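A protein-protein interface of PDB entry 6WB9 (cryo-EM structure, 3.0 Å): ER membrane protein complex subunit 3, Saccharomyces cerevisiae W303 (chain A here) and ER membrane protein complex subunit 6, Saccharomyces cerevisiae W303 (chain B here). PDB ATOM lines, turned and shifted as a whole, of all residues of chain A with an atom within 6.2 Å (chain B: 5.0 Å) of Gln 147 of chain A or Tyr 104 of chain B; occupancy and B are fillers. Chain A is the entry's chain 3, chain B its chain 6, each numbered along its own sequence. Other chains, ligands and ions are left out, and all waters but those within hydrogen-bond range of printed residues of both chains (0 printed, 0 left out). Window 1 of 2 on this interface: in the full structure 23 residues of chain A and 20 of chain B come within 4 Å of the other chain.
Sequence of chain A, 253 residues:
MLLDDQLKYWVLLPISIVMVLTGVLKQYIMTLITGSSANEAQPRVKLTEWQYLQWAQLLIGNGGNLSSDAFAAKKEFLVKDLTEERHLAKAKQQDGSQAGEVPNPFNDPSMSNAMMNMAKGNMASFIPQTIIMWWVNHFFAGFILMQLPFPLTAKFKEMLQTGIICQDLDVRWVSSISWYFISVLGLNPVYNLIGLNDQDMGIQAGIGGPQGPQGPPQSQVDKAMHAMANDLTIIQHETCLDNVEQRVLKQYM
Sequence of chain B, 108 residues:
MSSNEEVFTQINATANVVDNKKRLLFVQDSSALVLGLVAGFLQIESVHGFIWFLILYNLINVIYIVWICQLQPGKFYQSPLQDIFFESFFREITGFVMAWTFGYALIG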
ATOM      1  N   LEU A   3      -3.669  23.893   9.093  1.00  0.00           N
ATOM      2  CA  LEU A   3      -4.645  23.836  10.167  1.00  0.00           C
ATOM      3  C   LEU A   3      -5.104  22.401  10.396  1.00  0.00           C
ATOM      4  O   LEU A   3      -4.857  21.501   9.592  1.00  0.00           O
ATOM      5  CB  LEU A   3      -5.848  24.723   9.853  1.00  0.00           C
ATOM      6  CG  LEU A   3      -5.681  26.229  10.011  1.00  0.00           C
ATOM      7  CD1 LEU A   3      -6.949  26.916   9.591  1.00  0.00           C
ATOM      8  CD2 LEU A   3      -5.355  26.565  11.445  1.00  0.00           C
ATOM      9  N   LYS A   8     -12.081  22.259  11.717  1.00  0.00           N
ATOM     10  CA  LYS A   8     -13.154  22.560  10.775  1.00  0.00           C
ATOM     11  C   LYS A   8     -14.395  21.729  11.075  1.00  0.00           C
ATOM     12  O   LYS A   8     -15.478  22.277  11.311  1.00  0.00           O
ATOM     13  CB  LYS A   8     -12.681  22.318   9.340  1.00  0.00           C
ATOM     14  CG  LYS A   8     -12.058  23.529   8.652  1.00  0.00           C
ATOM     15  CD  LYS A   8     -10.627  23.782   9.095  1.00  0.00           C
ATOM     16  CE  LYS A   8      -9.934  24.776   8.181  1.00  0.00           C
ATOM     17  NZ  LYS A   8      -9.809  24.268   6.790  1.00  0.00           N
ATOM     18  N   ILE A 144      -7.115  29.260  15.680  1.00  0.00           N
ATOM     19  CA  ILE A 144      -7.496  29.764  14.369  1.00  0.00           C
ATOM     20  C   ILE A 144      -8.341  28.700  13.686  1.00  0.00           C
ATOM     21  O   ILE A 144      -7.883  27.574  13.466  1.00  0.00           O
ATOM     22  CB  ILE A 144      -6.259  30.116  13.532  1.00  0.00           C
ATOM     23  CG1 ILE A 144      -5.574  31.358  14.099  1.00  0.00           C
ATOM     24  CG2 ILE A 144      -6.630  30.320  12.081  1.00  0.00           C
ATOM     25  CD1 ILE A 144      -6.436  32.589  14.093  1.00  0.00           C
ATOM     26  N   LEU A 145      -9.583  29.049  13.362  1.00  0.00           N
ATOM     27  CA  LEU A 145     -10.493  28.072  12.780  1.00  0.00           C
ATOM     28  C   LEU A 145     -10.216  27.864  11.298  1.00  0.00           C
ATOM     29  O   LEU A 145     -10.091  26.723  10.842  1.00  0.00           O
ATOM     30  CB  LEU A 145     -11.943  28.508  13.006  1.00  0.00           C
ATOM     31  CG  LEU A 145     -13.055  28.027  12.068  1.00  0.00           C
ATOM     32  CD1 LEU A 145     -13.288  26.520  12.110  1.00  0.00           C
ATOM     33  CD2 LEU A 145     -14.331  28.764  12.396  1.00  0.00           C
ATOM     34  N   MET A 146     -10.120  28.941  10.530  1.00  0.00           N
ATOM     35  CA  MET A 146     -10.161  28.807   9.084  1.00  0.00           C
ATOM     36  C   MET A 146      -9.501  30.016   8.446  1.00  0.00           C
ATOM     37  O   MET A 146      -9.068  30.948   9.127  1.00  0.00           O
ATOM     38  CB  MET A 146     -11.600  28.665   8.601  1.00  0.00           C
ATOM     39  CG  MET A 146     -12.442  29.904   8.818  1.00  0.00           C
ATOM     40  SD  MET A 146     -14.176  29.649   8.438  1.00  0.00           S
ATOM     41  CE  MET A 146     -14.818  31.282   8.767  1.00  0.00           C
ATOM     42  N   GLN A 147      -9.444  29.994   7.120  1.00  0.00           N
ATOM     43  CA  GLN A 147      -8.953  31.106   6.323  1.00  0.00           C
ATOM     44  C   GLN A 147     -10.103  31.678   5.507  1.00  0.00           C
ATOM     45  O   GLN A 147     -10.833  30.929   4.849  1.00  0.00           O
ATOM     46  CB  GLN A 147      -7.821  30.662   5.400  1.00  0.00           C
ATOM     47  CG  GLN A 147      -7.168  31.800   4.655  1.00  0.00           C
ATOM     48  CD  GLN A 147      -6.124  31.330   3.675  1.00  0.00           C
ATOM     49  OE1 GLN A 147      -6.165  30.195   3.204  1.00  0.00           O
ATOM     50  NE2 GLN A 147      -5.176  32.200   3.362  1.00  0.00           N
ATOM     51  N   LEU A 148     -10.269  32.994   5.563  1.00  0.00           N
ATOM     52  CA  LEU A 148     -11.247  33.652   4.716  1.00  0.00           C
ATOM     53  C   LEU A 148     -10.781  33.618   3.261  1.00  0.00           C
ATOM     54  O   LEU A 148      -9.582  33.556   2.989  1.00  0.00           O
ATOM     55  CB  LEU A 148     -11.454  35.097   5.159  1.00  0.00           C
ATOM     56  CG  LEU A 148     -11.920  35.314   6.596  1.00  0.00           C
ATOM     57  CD1 LEU A 148     -12.162  36.789   6.867  1.00  0.00           C
ATOM     58  CD2 LEU A 148     -13.161  34.503   6.873  1.00  0.00           C
ATOM     59  N   PRO A 149     -11.708  33.631   2.305  1.00  0.00           N
ATOM     60  CA  PRO A 149     -11.320  33.770   0.899  1.00  0.00           C
ATOM     61  C   PRO A 149     -11.164  35.212   0.448  1.00  0.00           C
ATOM     62  O   PRO A 149     -10.831  35.443  -0.718  1.00  0.00           O
ATOM     63  CB  PRO A 149     -12.486  33.099   0.157  1.00  0.00           C
ATOM     64  CG  PRO A 149     -13.392  32.544   1.209  1.00  0.00           C
ATOM     65  CD  PRO A 149     -13.138  33.328   2.427  1.00  0.00           C
ATOM     66  N   ASP A 170      -2.018  37.493   9.211  1.00  0.00           N
ATOM     67  CA  ASP A 170      -2.816  38.444   8.455  1.00  0.00           C
ATOM     68  C   ASP A 170      -4.295  38.143   8.655  1.00  0.00           C
ATOM     69  O   ASP A 170      -4.677  37.077   9.141  1.00  0.00           O
ATOM     70  CB  ASP A 170      -2.459  38.407   6.972  1.00  0.00           C
ATOM     71  CG  ASP A 170      -2.935  37.148   6.291  1.00  0.00           C
ATOM     72  OD1 ASP A 170      -2.751  36.059   6.864  1.00  0.00           O
ATOM     73  OD2 ASP A 170      -3.495  37.249   5.181  1.00  0.00           O
ATOM     74  N   ARG A 172      -6.874  36.948   7.261  1.00  0.00           N
ATOM     75  CA  ARG A 172      -7.568  35.862   6.600  1.00  0.00           C
ATOM     76  C   ARG A 172      -7.752  34.708   7.559  1.00  0.00           C
ATOM     77  O   ARG A 172      -8.823  34.107   7.597  1.00  0.00           O
ATOM     78  CB  ARG A 172      -6.792  35.399   5.365  1.00  0.00           C
ATOM     79  CG  ARG A 172      -6.653  36.440   4.279  1.00  0.00           C
ATOM     80  CD  ARG A 172      -7.701  36.247   3.220  1.00  0.00           C
ATOM     81  NE  ARG A 172      -7.558  34.966   2.539  1.00  0.00           N
ATOM     82  CZ  ARG A 172      -7.028  34.819   1.332  1.00  0.00           C
ATOM     83  NH1 ARG A 172      -6.591  35.876   0.667  1.00  0.00           N
ATOM     84  NH2 ARG A 172      -6.942  33.617   0.787  1.00  0.00           N
ATOM     85  N   TRP A 173      -6.743  34.433   8.382  1.00  0.00           N
ATOM     86  CA  TRP A 173      -6.805  33.378   9.379  1.00  0.00           C
ATOM     87  C   TRP A 173      -7.549  33.902  10.594  1.00  0.00           C
ATOM     88  O   TRP A 173      -7.088  34.832  11.260  1.00  0.00           O
ATOM     89  CB  TRP A 173      -5.401  32.919   9.750  1.00  0.00           C
ATOM     90  CG  TRP A 173      -4.609  32.512   8.570  1.00  0.00           C
ATOM     91  CD1 TRP A 173      -3.719  33.273   7.885  1.00  0.00           C
ATOM     92  CD2 TRP A 173      -4.644  31.244   7.912  1.00  0.00           C
ATOM     93  NE1 TRP A 173      -3.188  32.560   6.843  1.00  0.00           N
ATOM     94  CE2 TRP A 173      -3.742  31.308   6.839  1.00  0.00           C
ATOM     95  CE3 TRP A 173      -5.349  30.060   8.130  1.00  0.00           C
ATOM     96  CZ2 TRP A 173      -3.526  30.236   5.984  1.00  0.00           C
ATOM     97  CZ3 TRP A 173      -5.133  28.998   7.281  1.00  0.00           C
ATOM     98  CH2 TRP A 173      -4.231  29.091   6.222  1.00  0.00           C
ATOM     99  N   VAL A 174      -8.699  33.299  10.878  1.00  0.00           N
ATOM    100  CA  VAL A 174      -9.690  33.879  11.765  1.00  0.00           C
ATOM    101  C   VAL A 174     -10.112  32.850  12.803  1.00  0.00           C
ATOM    102  O   VAL A 174      -9.994  31.641  12.601  1.00  0.00           O
ATOM    103  CB  VAL A 174     -10.909  34.374  10.972  1.00  0.00           C
ATOM    104  CG1 VAL A 174     -10.584  35.639  10.214  1.00  0.00           C
ATOM    105  CG2 VAL A 174     -11.356  33.303  10.003  1.00  0.00           C
ATOM    106  N   ALA B  39     -18.140  28.218  -5.169  1.00  0.00           N
ATOM    107  CA  ALA B  39     -16.982  29.094  -5.034  1.00  0.00           C
ATOM    108  C   ALA B  39     -16.049  28.656  -3.914  1.00  0.00           C
ATOM    109  O   ALA B  39     -14.869  29.011  -3.936  1.00  0.00           O
ATOM    110  CB  ALA B  39     -17.430  30.532  -4.789  1.00  0.00           C
ATOM    111  N   GLY B  40     -16.552  27.911  -2.929  1.00  0.00           N
ATOM    112  CA  GLY B  40     -15.668  27.314  -1.947  1.00  0.00           C
ATOM    113  C   GLY B  40     -15.046  26.014  -2.404  1.00  0.00           C
ATOM    114  O   GLY B  40     -13.920  25.698  -2.012  1.00  0.00           O
ATOM    115  N   GLN B  43     -12.188  26.892  -4.598  1.00  0.00           N
ATOM    116  CA  GLN B  43     -11.202  27.675  -3.847  1.00  0.00           C
ATOM    117  C   GLN B  43     -10.899  29.001  -4.545  1.00  0.00           C
ATOM    118  O   GLN B  43      -9.768  29.292  -4.935  1.00  0.00           O
ATOM    119  CB  GLN B  43      -9.927  26.865  -3.595  1.00  0.00           C
ATOM    120  CG  GLN B  43     -10.134  25.681  -2.676  1.00  0.00           C
ATOM    121  CD  GLN B  43     -10.014  26.054  -1.220  1.00  0.00           C
ATOM    122  OE1 GLN B  43      -9.009  26.621  -0.795  1.00  0.00           O
ATOM    123  NE2 GLN B  43     -11.038  25.742  -0.446  1.00  0.00           N
ATOM    124  N   ILE B  44     -11.945  29.800  -4.703  1.00  0.00           N
ATOM    125  CA  ILE B  44     -11.850  31.082  -5.389  1.00  0.00           C
ATOM    126  C   ILE B  44     -11.538  32.161  -4.362  1.00  0.00           C
ATOM    127  O   ILE B  44     -12.132  32.189  -3.279  1.00  0.00           O
ATOM    128  CB  ILE B  44     -13.149  31.391  -6.151  1.00  0.00           C
ATOM    129  CG1 ILE B  44     -13.576  30.180  -6.978  1.00  0.00           C
ATOM    130  CG2 ILE B  44     -12.949  32.558  -7.072  1.00  0.00           C
ATOM    131  CD1 ILE B  44     -14.797  30.411  -7.837  1.00  0.00           C
ATOM    132  N   GLU B  45     -10.595  33.041  -4.692  1.00  0.00           N
ATOM    133  CA  GLU B  45     -10.189  34.121  -3.805  1.00  0.00           C
ATOM    134  C   GLU B  45     -11.110  35.323  -4.005  1.00  0.00           C
ATOM    135  O   GLU B  45     -12.141  35.230  -4.670  1.00  0.00           O
ATOM    136  CB  GLU B  45      -8.721  34.470  -4.030  1.00  0.00           C
ATOM    137  CG  GLU B  45      -7.761  33.729  -3.110  1.00  0.00           C
ATOM    138  CD  GLU B  45      -7.743  32.236  -3.357  1.00  0.00           C
ATOM    139  OE1 GLU B  45      -7.759  31.825  -4.536  1.00  0.00           O
ATOM    140  OE2 GLU B  45      -7.719  31.470  -2.373  1.00  0.00           O
ATOM    141  N   ALA B  99     -21.757  30.838   2.719  1.00  0.00           N
ATOM    142  CA  ALA B  99     -21.523  29.545   2.081  1.00  0.00           C
ATOM    143  C   ALA B  99     -20.148  29.478   1.431  1.00  0.00           C
ATOM    144  O   ALA B  99     -19.564  28.395   1.330  1.00  0.00           O
ATOM    145  CB  ALA B  99     -22.614  29.264   1.053  1.00  0.00           C
ATOM    146  N   TRP B 100     -19.603  30.628   1.034  1.00  0.00           N
ATOM    147  CA  TRP B 100     -18.272  30.717   0.452  1.00  0.00           C
ATOM    148  C   TRP B 100     -17.207  30.406   1.486  1.00  0.00           C
ATOM    149  O   TRP B 100     -16.287  29.629   1.223  1.00  0.00           O
ATOM    150  CB  TRP B 100     -18.079  32.121  -0.108  1.00  0.00           C
ATOM    151  CG  TRP B 100     -16.879  32.338  -0.942  1.00  0.00           C
ATOM    152  CD1 TRP B 100     -16.115  31.397  -1.555  1.00  0.00           C
ATOM    153  CD2 TRP B 100     -16.305  33.601  -1.272  1.00  0.00           C
ATOM    154  NE1 TRP B 100     -15.096  31.998  -2.248  1.00  0.00           N
ATOM    155  CE2 TRP B 100     -15.193  33.354  -2.088  1.00  0.00           C
ATOM    156  CE3 TRP B 100     -16.624  34.921  -0.948  1.00  0.00           C
ATOM    157  CZ2 TRP B 100     -14.402  34.374  -2.590  1.00  0.00           C
ATOM    158  CZ3 TRP B 100     -15.839  35.931  -1.447  1.00  0.00           C
ATOM    159  CH2 TRP B 100     -14.740  35.655  -2.258  1.00  0.00           C
ATOM    160  N   THR B 101     -17.321  31.009   2.671  1.00  0.00           N
ATOM    161  CA  THR B 101     -16.406  30.709   3.762  1.00  0.00           C
ATOM    162  C   THR B 101     -16.556  29.274   4.241  1.00  0.00           C
ATOM    163  O   THR B 101     -15.551  28.632   4.557  1.00  0.00           O
ATOM    164  CB  THR B 101     -16.634  31.678   4.916  1.00  0.00           C
ATOM    165  OG1 THR B 101     -18.037  31.804   5.148  1.00  0.00           O
ATOM    166  CG2 THR B 101     -16.089  33.037   4.581  1.00  0.00           C
ATOM    167  N   PHE B 102     -17.786  28.744   4.250  1.00  0.00           N
ATOM    168  CA  PHE B 102     -18.004  27.355   4.650  1.00  0.00           C
ATOM    169  C   PHE B 102     -17.345  26.382   3.678  1.00  0.00           C
ATOM    170  O   PHE B 102     -16.626  25.469   4.095  1.00  0.00           O
ATOM    171  CB  PHE B 102     -19.503  27.075   4.755  1.00  0.00           C
ATOM    172  CG  PHE B 102     -19.830  25.719   5.304  1.00  0.00           C
ATOM    173  CD1 PHE B 102     -19.810  25.493   6.668  1.00  0.00           C
ATOM    174  CD2 PHE B 102     -20.168  24.673   4.459  1.00  0.00           C
ATOM    175  CE1 PHE B 102     -20.113  24.252   7.180  1.00  0.00           C
ATOM    176  CE2 PHE B 102     -20.468  23.429   4.964  1.00  0.00           C
ATOM    177  CZ  PHE B 102     -20.442  23.218   6.327  1.00  0.00           C
ATOM    178  N   GLY B 103     -17.568  26.571   2.376  1.00  0.00           N
ATOM    179  CA  GLY B 103     -16.969  25.687   1.395  1.00  0.00           C
ATOM    180  C   GLY B 103     -15.474  25.872   1.250  1.00  0.00           C
ATOM    181  O   GLY B 103     -14.754  24.908   0.991  1.00  0.00           O
ATOM    182  N   TYR B 104     -14.986  27.099   1.421  1.00  0.00           N
ATOM    183  CA  TYR B 104     -13.558  27.364   1.310  1.00  0.00           C
ATOM    184  C   TYR B 104     -12.806  26.810   2.508  1.00  0.00           C
ATOM    185  O   TYR B 104     -11.666  26.354   2.377  1.00  0.00           O
ATOM    186  CB  TYR B 104     -13.337  28.868   1.177  1.00  0.00           C
ATOM    187  CG  TYR B 104     -11.943  29.284   0.786  1.00  0.00           C
ATOM    188  CD1 TYR B 104     -11.562  29.328  -0.546  1.00  0.00           C
ATOM    189  CD2 TYR B 104     -11.014  29.659   1.748  1.00  0.00           C
ATOM    190  CE1 TYR B 104     -10.292  29.716  -0.909  1.00  0.00           C
ATOM    191  CE2 TYR B 104      -9.741  30.048   1.394  1.00  0.00           C
ATOM    192  CZ  TYR B 104      -9.387  30.075   0.063  1.00  0.00           C
ATOM    193  OH  TYR B 104      -8.119  30.462  -0.297  1.00  0.00           O
ATOM    194  N   ALA B 105     -13.430  26.840   3.687  1.00  0.00           N
ATOM    195  CA  ALA B 105     -12.815  26.250   4.862  1.00  0.00           C
ATOM    196  C   ALA B 105     -12.920  24.735   4.853  1.00  0.00           C
ATOM    197  O   ALA B 105     -12.024  24.051   5.355  1.00  0.00           O
ATOM    198  CB  ALA B 105     -13.469  26.816   6.111  1.00  0.00           C
ATOM    199  N   LEU B 106     -13.998  24.191   4.291  1.00  0.00           N
ATOM    200  CA  LEU B 106     -14.193  22.749   4.276  1.00  0.00           C
ATOM    201  C   LEU B 106     -13.380  22.046   3.199  1.00  0.00           C
ATOM    202  O   LEU B 106     -13.292  20.814   3.225  1.00  0.00           O
ATOM    203  CB  LEU B 106     -15.675  22.427   4.089  1.00  0.00           C
ATOM    204  CG  LEU B 106     -16.216  21.277   4.932  1.00  0.00           C
ATOM    205  CD1 LEU B 106     -16.100  21.611   6.407  1.00  0.00           C
ATOM    206  CD2 LEU B 106     -17.653  20.984   4.562  1.00  0.00           C
ATOM    207  N   ILE B 107     -12.796  22.779   2.259  1.00  0.00           N
ATOM    208  CA  ILE B 107     -11.980  22.168   1.217  1.00  0.00           C
ATOM    209  C   ILE B 107     -10.510  22.482   1.456  1.00  0.00           C
ATOM    210  O   ILE B 107     -10.151  23.612   1.785  1.00  0.00           O
ATOM    211  CB  ILE B 107     -12.415  22.633  -0.189  1.00  0.00           C
ATOM    212  CG1 ILE B 107     -13.845  22.183  -0.511  1.00  0.00           C
ATOM    213  CG2 ILE B 107     -11.444  22.142  -1.243  1.00  0.00           C
ATOM    214  CD1 ILE B 107     -14.157  20.764  -0.165  1.00  0.00           C
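O of Ala 105 of chain B sits at hydrogen-bond distance from NZ of Lys 8 of chain A, at 2.6 Å.
The guanidinium group (NH2) of Arg 172 of chain A is in salt-bridge range of the side-chain carboxylate (OE2) of Glu 45 of chain B, 3.9 Å away.
O of Ile 44 of chain B is in hydrogen-bond range of NE1 of Trp 100 of chain B (3.1 Å).
The indole nitrogen (NE1) of Trp 100 of chain B sits at hydrogen-bond distance from the backbone carbonyl oxygen (O) of Ala 39 of chain B.
The backbone NH (N) of Ile 44 of chain B lies within hydrogen-bond range of the backbone carbonyl oxygen (O) of Ala 39 of chain B (3.1 Å).
The backbone NH (N) of Val 174 of chain A lies within hydrogen-bond range of the backbone carbonyl oxygen (O) of Met 146 of chain A (3.0 Å).
The side-chain amide nitrogen of Gln 43 of chain B is in hydrogen-bond range of the backbone carbonyl oxygen of Tyr 104 of chain B (3.0 Å).
The guanidinium group (NH2) of Arg 172 of chain A lies close to the side-chain amide nitrogen (NE2) of Gln 147 of chain A.
Met 146 of chain A touches Ala 105 of chain B.
Gln 147 of chain A touches Tyr 104 of chain B (O to CD2, 3.4 Å).
Leu 148 of chain A touches Thr 101 of chain B.
Tyr 104 of chain B touches Leu 148 of chain A (CE2 to O, 3.9 Å).
Pro 149 of chain A touches Ile 44 of chain B (CB to O, 3.6 Å).
O of Pro 149 of chain A touches C of Glu 45 of chain B, 3.3 Å away.
Trp 100 of chain B touches Pro 149 of chain A.
Thr 101 of chain B touches Pro 149 of chain A.
Pro 149 of chain A touches Tyr 104 of chain B (CG to CG, 3.6 Å).
Tyr 104 of chain B touches Arg 172 of chain A.
Tyr 104 of chain B touches just these residues of chain A: Gln 147 (3.4 Å), Leu 148 (3.9 Å), Pro 149 (3.6 Å) and Arg 172 (3.5 Å).
Of the printed residues of chain B, Pro 149 of chain A touches Ile 44, Glu 45, Trp 100, Thr 101 and Tyr 104.
Printed residues of chain A within 4 Å of Thr 101 of chain B: Leu 148 (3.997 Å) and Pro 149 (3.7 Å).
Ile 144 of chain A touches none of the printed residues of chain B.
Asp 170 of chain A touches none of the printed residues of chain B.
The nearest printed residue of chain B that does not touch Gln 147 of chain A is Ala 105 of chain B (5.0 Å).
The nearest residue of chain A that does not touch Tyr 104 of chain B is Lys 8 of chain A (5.2 Å).
Among the printed residues, Asp or Glu carboxylates within 4 Å of a Lys or Arg side-chain nitrogen of the other chain: Arg 172 of chain A with Glu 45 of chain B (3.9 Å).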
